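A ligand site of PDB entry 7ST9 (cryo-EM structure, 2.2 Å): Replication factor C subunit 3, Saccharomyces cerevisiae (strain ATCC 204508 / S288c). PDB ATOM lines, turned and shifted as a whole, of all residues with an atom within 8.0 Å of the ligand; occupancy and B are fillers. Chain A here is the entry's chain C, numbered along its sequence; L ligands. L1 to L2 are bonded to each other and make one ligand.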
ATOM      1  N   LEU A 252     -10.022  21.770  21.411  1.00  0.00           N
ATOM      2  CA  LEU A 252     -11.253  21.855  20.632  1.00  0.00           C
ATOM      3  C   LEU A 252     -11.042  22.297  19.192  1.00  0.00           C
ATOM      4  O   LEU A 252     -11.999  22.233  18.407  1.00  0.00           O
ATOM      5  CB  LEU A 252     -12.226  22.831  21.308  1.00  0.00           C
ATOM      6  CG  LEU A 252     -12.771  22.415  22.678  1.00  0.00           C
ATOM      7  CD1 LEU A 252     -13.584  23.546  23.291  1.00  0.00           C
ATOM      8  CD2 LEU A 252     -13.619  21.156  22.564  1.00  0.00           C
ATOM      9  N   TYR A 288     -20.408  26.668  29.138  1.00  0.00           N
ATOM     10  CA  TYR A 288     -20.549  26.539  27.687  1.00  0.00           C
ATOM     11  C   TYR A 288     -21.995  26.264  27.310  1.00  0.00           C
ATOM     12  O   TYR A 288     -22.711  25.524  28.001  1.00  0.00           O
ATOM     13  CB  TYR A 288     -19.654  25.422  27.161  1.00  0.00           C
ATOM     14  CG  TYR A 288     -18.380  25.916  26.502  1.00  0.00           C
ATOM     15  CD1 TYR A 288     -17.559  26.835  27.142  1.00  0.00           C
ATOM     16  CD2 TYR A 288     -18.003  25.461  25.250  1.00  0.00           C
ATOM     17  CE1 TYR A 288     -16.390  27.288  26.543  1.00  0.00           C
ATOM     18  CE2 TYR A 288     -16.839  25.904  24.644  1.00  0.00           C
ATOM     19  CZ  TYR A 288     -16.046  26.811  25.297  1.00  0.00           C
ATOM     20  OH  TYR A 288     -14.891  27.263  24.698  1.00  0.00           O
ATOM     21  N   GLU A 289     -22.436  26.864  26.209  1.00  0.00           N
ATOM     22  CA  GLU A 289     -23.775  26.642  25.672  1.00  0.00           C
ATOM     23  C   GLU A 289     -23.716  25.461  24.702  1.00  0.00           C
ATOM     24  O   GLU A 289     -23.176  25.588  23.599  1.00  0.00           O
ATOM     25  CB  GLU A 289     -24.299  27.895  24.993  1.00  0.00           C
ATOM     26  CG  GLU A 289     -25.742  27.794  24.522  1.00  0.00           C
ATOM     27  CD  GLU A 289     -26.258  29.095  23.930  1.00  0.00           C
ATOM     28  OE1 GLU A 289     -25.483  30.072  23.877  1.00  0.00           O
ATOM     29  OE2 GLU A 289     -27.437  29.143  23.532  1.00  0.00           O
ATOM     30  N   LEU A 290     -24.281  24.330  25.115  1.00  0.00           N
ATOM     31  CA  LEU A 290     -24.243  23.102  24.319  1.00  0.00           C
ATOM     32  C   LEU A 290     -25.601  22.872  23.676  1.00  0.00           C
ATOM     33  O   LEU A 290     -26.622  22.840  24.376  1.00  0.00           O
ATOM     34  CB  LEU A 290     -23.857  21.913  25.195  1.00  0.00           C
ATOM     35  CG  LEU A 290     -22.488  21.992  25.877  1.00  0.00           C
ATOM     36  CD1 LEU A 290     -22.246  20.751  26.727  1.00  0.00           C
ATOM     37  CD2 LEU A 290     -21.372  22.172  24.858  1.00  0.00           C
ATOM     38  N   GLN A 291     -25.616  22.720  22.355  1.00  0.00           N
ATOM     39  CA  GLN A 291     -26.853  22.421  21.641  1.00  0.00           C
ATOM     40  C   GLN A 291     -27.196  20.938  21.651  1.00  0.00           C
ATOM     41  O   GLN A 291     -28.332  20.585  21.340  1.00  0.00           O
ATOM     42  CB  GLN A 291     -26.745  22.915  20.187  1.00  0.00           C
ATOM     43  CG  GLN A 291     -25.555  22.361  19.408  1.00  0.00           C
ATOM     44  CD  GLN A 291     -24.849  23.436  18.600  1.00  0.00           C
ATOM     45  OE1 GLN A 291     -25.469  24.403  18.151  1.00  0.00           O
ATOM     46  NE2 GLN A 291     -23.548  23.284  18.431  1.00  0.00           N
ATOM     47  N   ASN A 292     -26.249  20.080  22.004  1.00  0.00           N
ATOM     48  CA  ASN A 292     -26.471  18.643  22.131  1.00  0.00           C
ATOM     49  C   ASN A 292     -26.240  18.257  23.588  1.00  0.00           C
ATOM     50  O   ASN A 292     -25.185  18.575  24.157  1.00  0.00           O
ATOM     51  CB  ASN A 292     -25.530  17.863  21.212  1.00  0.00           C
ATOM     52  CG  ASN A 292     -26.000  16.437  20.981  1.00  0.00           C
ATOM     53  OD1 ASN A 292     -27.007  15.998  21.548  1.00  0.00           O
ATOM     54  ND2 ASN A 292     -25.270  15.698  20.152  1.00  0.00           N
ATOM     55  N   GLU A 293     -27.213  17.569  24.176  1.00  0.00           N
ATOM     56  CA  GLU A 293     -27.135  17.252  25.597  1.00  0.00           C
ATOM     57  C   GLU A 293     -26.312  16.005  25.879  1.00  0.00           C
ATOM     58  O   GLU A 293     -25.766  15.875  26.983  1.00  0.00           O
ATOM     59  CB  GLU A 293     -28.540  17.081  26.186  1.00  0.00           C
ATOM     60  CG  GLU A 293     -28.538  16.716  27.653  1.00  0.00           C
ATOM     61  CD  GLU A 293     -28.752  15.237  27.899  1.00  0.00           C
ATOM     62  OE1 GLU A 293     -28.596  14.445  26.943  1.00  0.00           O
ATOM     63  OE2 GLU A 293     -29.060  14.857  29.042  1.00  0.00           O
ATOM     64  N   GLU A 294     -26.203  15.089  24.918  1.00  0.00           N
ATOM     65  CA  GLU A 294     -25.361  13.905  25.124  1.00  0.00           C
ATOM     66  C   GLU A 294     -23.901  14.307  25.329  1.00  0.00           C
ATOM     67  O   GLU A 294     -23.158  13.593  26.023  1.00  0.00           O
ATOM     68  CB  GLU A 294     -25.480  12.968  23.925  1.00  0.00           C
ATOM     69  CG  GLU A 294     -25.827  11.524  24.297  1.00  0.00           C
ATOM     70  CD  GLU A 294     -27.135  11.417  25.052  1.00  0.00           C
ATOM     71  OE1 GLU A 294     -28.098  12.134  24.680  1.00  0.00           O
ATOM     72  OE2 GLU A 294     -27.208  10.629  26.016  1.00  0.00           O
ATOM     73  N   THR A 295     -23.481  15.432  24.751  1.00  0.00           N
ATOM     74  CA  THR A 295     -22.118  15.907  24.949  1.00  0.00           C
ATOM     75  C   THR A 295     -21.831  16.157  26.421  1.00  0.00           C
ATOM     76  O   THR A 295     -20.775  15.765  26.925  1.00  0.00           O
ATOM     77  CB  THR A 295     -21.889  17.184  24.131  1.00  0.00           C
ATOM     78  OG1 THR A 295     -22.104  16.907  22.745  1.00  0.00           O
ATOM     79  CG2 THR A 295     -20.473  17.703  24.346  1.00  0.00           C
ATOM     80  N   ARG A 296     -22.770  16.793  27.122  1.00  0.00           N
ATOM     81  CA  ARG A 296     -22.595  17.036  28.549  1.00  0.00           C
ATOM     82  C   ARG A 296     -22.494  15.716  29.316  1.00  0.00           C
ATOM     83  O   ARG A 296     -21.659  15.575  30.213  1.00  0.00           O
ATOM     84  CB  ARG A 296     -23.759  17.870  29.082  1.00  0.00           C
ATOM     85  CG  ARG A 296     -23.639  18.257  30.554  1.00  0.00           C
ATOM     86  CD  ARG A 296     -22.647  19.374  30.772  1.00  0.00           C
ATOM     87  NE  ARG A 296     -23.104  20.639  30.195  1.00  0.00           N
ATOM     88  CZ  ARG A 296     -22.348  21.708  30.031  1.00  0.00           C
ATOM     89  NH1 ARG A 296     -21.081  21.728  30.412  1.00  0.00           N
ATOM     90  NH2 ARG A 296     -22.877  22.806  29.489  1.00  0.00           N
ATOM     91  N   LYS A 328     -12.522  15.541  22.968  1.00  0.00           N
ATOM     92  CA  LYS A 328     -12.736  15.527  21.527  1.00  0.00           C
ATOM     93  C   LYS A 328     -13.920  14.641  21.149  1.00  0.00           C
ATOM     94  O   LYS A 328     -14.778  15.037  20.359  1.00  0.00           O
ATOM     95  CB  LYS A 328     -11.469  15.058  20.809  1.00  0.00           C
ATOM     96  CG  LYS A 328     -10.381  16.121  20.730  1.00  0.00           C
ATOM     97  CD  LYS A 328      -9.102  15.560  20.116  1.00  0.00           C
ATOM     98  CE  LYS A 328      -8.013  16.612  20.051  1.00  0.00           C
ATOM     99  NZ  LYS A 328      -8.292  17.645  19.009  1.00  0.00           N
ATOM    100  N   ALA A 329     -13.987  13.444  21.726  1.00  0.00           N
ATOM    101  CA  ALA A 329     -15.085  12.532  21.420  1.00  0.00           C
ATOM    102  C   ALA A 329     -16.419  13.114  21.878  1.00  0.00           C
ATOM    103  O   ALA A 329     -17.423  13.004  21.168  1.00  0.00           O
ATOM    104  CB  ALA A 329     -14.843  11.167  22.068  1.00  0.00           C
ATOM    105  N   SER A 330     -16.445  13.718  23.064  1.00  0.00           N
ATOM    106  CA  SER A 330     -17.688  14.306  23.560  1.00  0.00           C
ATOM    107  C   SER A 330     -18.173  15.409  22.629  1.00  0.00           C
ATOM    108  O   SER A 330     -19.364  15.494  22.325  1.00  0.00           O
ATOM    109  CB  SER A 330     -17.479  14.853  24.968  1.00  0.00           C
ATOM    110  OG  SER A 330     -17.786  13.876  25.943  1.00  0.00           O
ATOM    111  N   PHE A 331     -17.257  16.260  22.158  1.00  0.00           N
ATOM    112  CA  PHE A 331     -17.665  17.357  21.293  1.00  0.00           C
ATOM    113  C   PHE A 331     -17.874  16.922  19.839  1.00  0.00           C
ATOM    114  O   PHE A 331     -18.388  17.718  19.047  1.00  0.00           O
ATOM    115  CB  PHE A 331     -16.635  18.482  21.350  1.00  0.00           C
ATOM    116  CG  PHE A 331     -16.984  19.559  22.325  1.00  0.00           C
ATOM    117  CD1 PHE A 331     -17.866  20.572  21.985  1.00  0.00           C
ATOM    118  CD2 PHE A 331     -16.446  19.563  23.609  1.00  0.00           C
ATOM    119  CE1 PHE A 331     -18.192  21.563  22.887  1.00  0.00           C
ATOM    120  CE2 PHE A 331     -16.773  20.554  24.511  1.00  0.00           C
ATOM    121  CZ  PHE A 331     -17.646  21.559  24.150  1.00  0.00           C
ATOM    122  N   GLU A 332     -17.485  15.699  19.482  1.00  0.00           N
ATOM    123  CA  GLU A 332     -17.756  15.206  18.131  1.00  0.00           C
ATOM    124  C   GLU A 332     -19.218  14.824  17.926  1.00  0.00           C
ATOM    125  O   GLU A 332     -19.659  14.723  16.789  1.00  0.00           O
ATOM    126  CB  GLU A 332     -16.865  14.002  17.821  1.00  0.00           C
ATOM    127  CG  GLU A 332     -15.498  14.359  17.287  1.00  0.00           C
ATOM    128  CD  GLU A 332     -14.616  13.152  17.055  1.00  0.00           C
ATOM    129  OE1 GLU A 332     -15.091  12.013  17.285  1.00  0.00           O
ATOM    130  OE2 GLU A 332     -13.450  13.327  16.652  1.00  0.00           O
ATOM    131  N   ASN A 333     -19.964  14.622  19.009  1.00  0.00           N
ATOM    132  CA  ASN A 333     -21.371  14.231  18.904  1.00  0.00           C
ATOM    133  C   ASN A 333     -22.170  15.235  18.084  1.00  0.00           C
ATOM    134  O   ASN A 333     -23.249  15.659  18.486  1.00  0.00           O
ATOM    135  CB  ASN A 333     -22.001  14.079  20.287  1.00  0.00           C
ATOM    136  CG  ASN A 333     -21.177  13.184  21.203  1.00  0.00           C
ATOM    137  OD1 ASN A 333     -20.464  12.291  20.743  1.00  0.00           O
ATOM    138  ND2 ASN A 333     -21.289  13.407  22.503  1.00  0.00           N
HETATM  139  N1  LIG L   1     -21.146  17.901  18.947  1.00  0.00           N
HETATM  140  C1  LIG L   1     -22.102  18.993  18.785  1.00  0.00           C
HETATM  141  C2  LIG L   1     -22.702  19.007  17.379  1.00  0.00           C
HETATM  142  O1  LIG L   1     -23.783  19.549  17.169  1.00  0.00           O
HETATM  143  C3  LIG L   1     -21.421  20.344  19.082  1.00  0.00           C
HETATM  144  C4  LIG L   1     -21.532  20.784  20.523  1.00  0.00           C
HETATM  145  C5  LIG L   1     -21.263  22.265  20.695  1.00  0.00           C
HETATM  146  O2  LIG L   1     -20.581  22.858  19.836  1.00  0.00           O
HETATM  147  O3  LIG L   1     -21.730  22.850  21.695  1.00  0.00           O
HETATM  148  N1  LG2 L   2     -21.987  18.411  16.434  1.00  0.00           N
HETATM  149  C1  LG2 L   2     -22.448  18.355  15.050  1.00  0.00           C
HETATM  150  C2  LG2 L   2     -23.770  17.610  14.950  1.00  0.00           C
HETATM  151  O1  LG2 L   2     -24.336  17.456  13.865  1.00  0.00           O
HETATM  152  C3  LG2 L   2     -21.416  17.682  14.137  1.00  0.00           C
HETATM  153  O2  LG2 L   2     -21.224  16.320  14.543  1.00  0.00           O
HETATM  154  C4  LG2 L   2     -20.077  18.410  14.194  1.00  0.00           C
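N1 of LIG L1 lies within hydrogen-bond range of O of Phe 331 (2.8 Å). O of Asn 333 sits close to N1 of LIG L1. O of Glu 332 lies within hydrogen-bond range of O2 of LG2 L2, 3.2 Å away. The backbone NH (N) of Asn 333 sits close to a nitrogen (N1) of LIG L1. NE2 of Gln 291 sits at hydrogen-bond distance from O2 of LIG L1, 3.3 Å away.
The backbone carbonyl oxygen (O) of Asn 333 lies within hydrogen-bond range of the side-chain amide nitrogen (ND2) of Asn 292 (2.6 Å). ND2 of Asn 333 lies within hydrogen-bond range of O of Ser 330 (2.8 Å). OD1 of Asn 333 lies close to O of Ala 329.
Residues that only touch the ligand: Glu 289 and Leu 290. Hydrophobic or aromatic side chains that line the ligand: Leu 290 and Phe 331. Within 4 Å of the ligand: Glu 289, Leu 290, Gln 291, Phe 331, Glu 332 and Asn 333.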
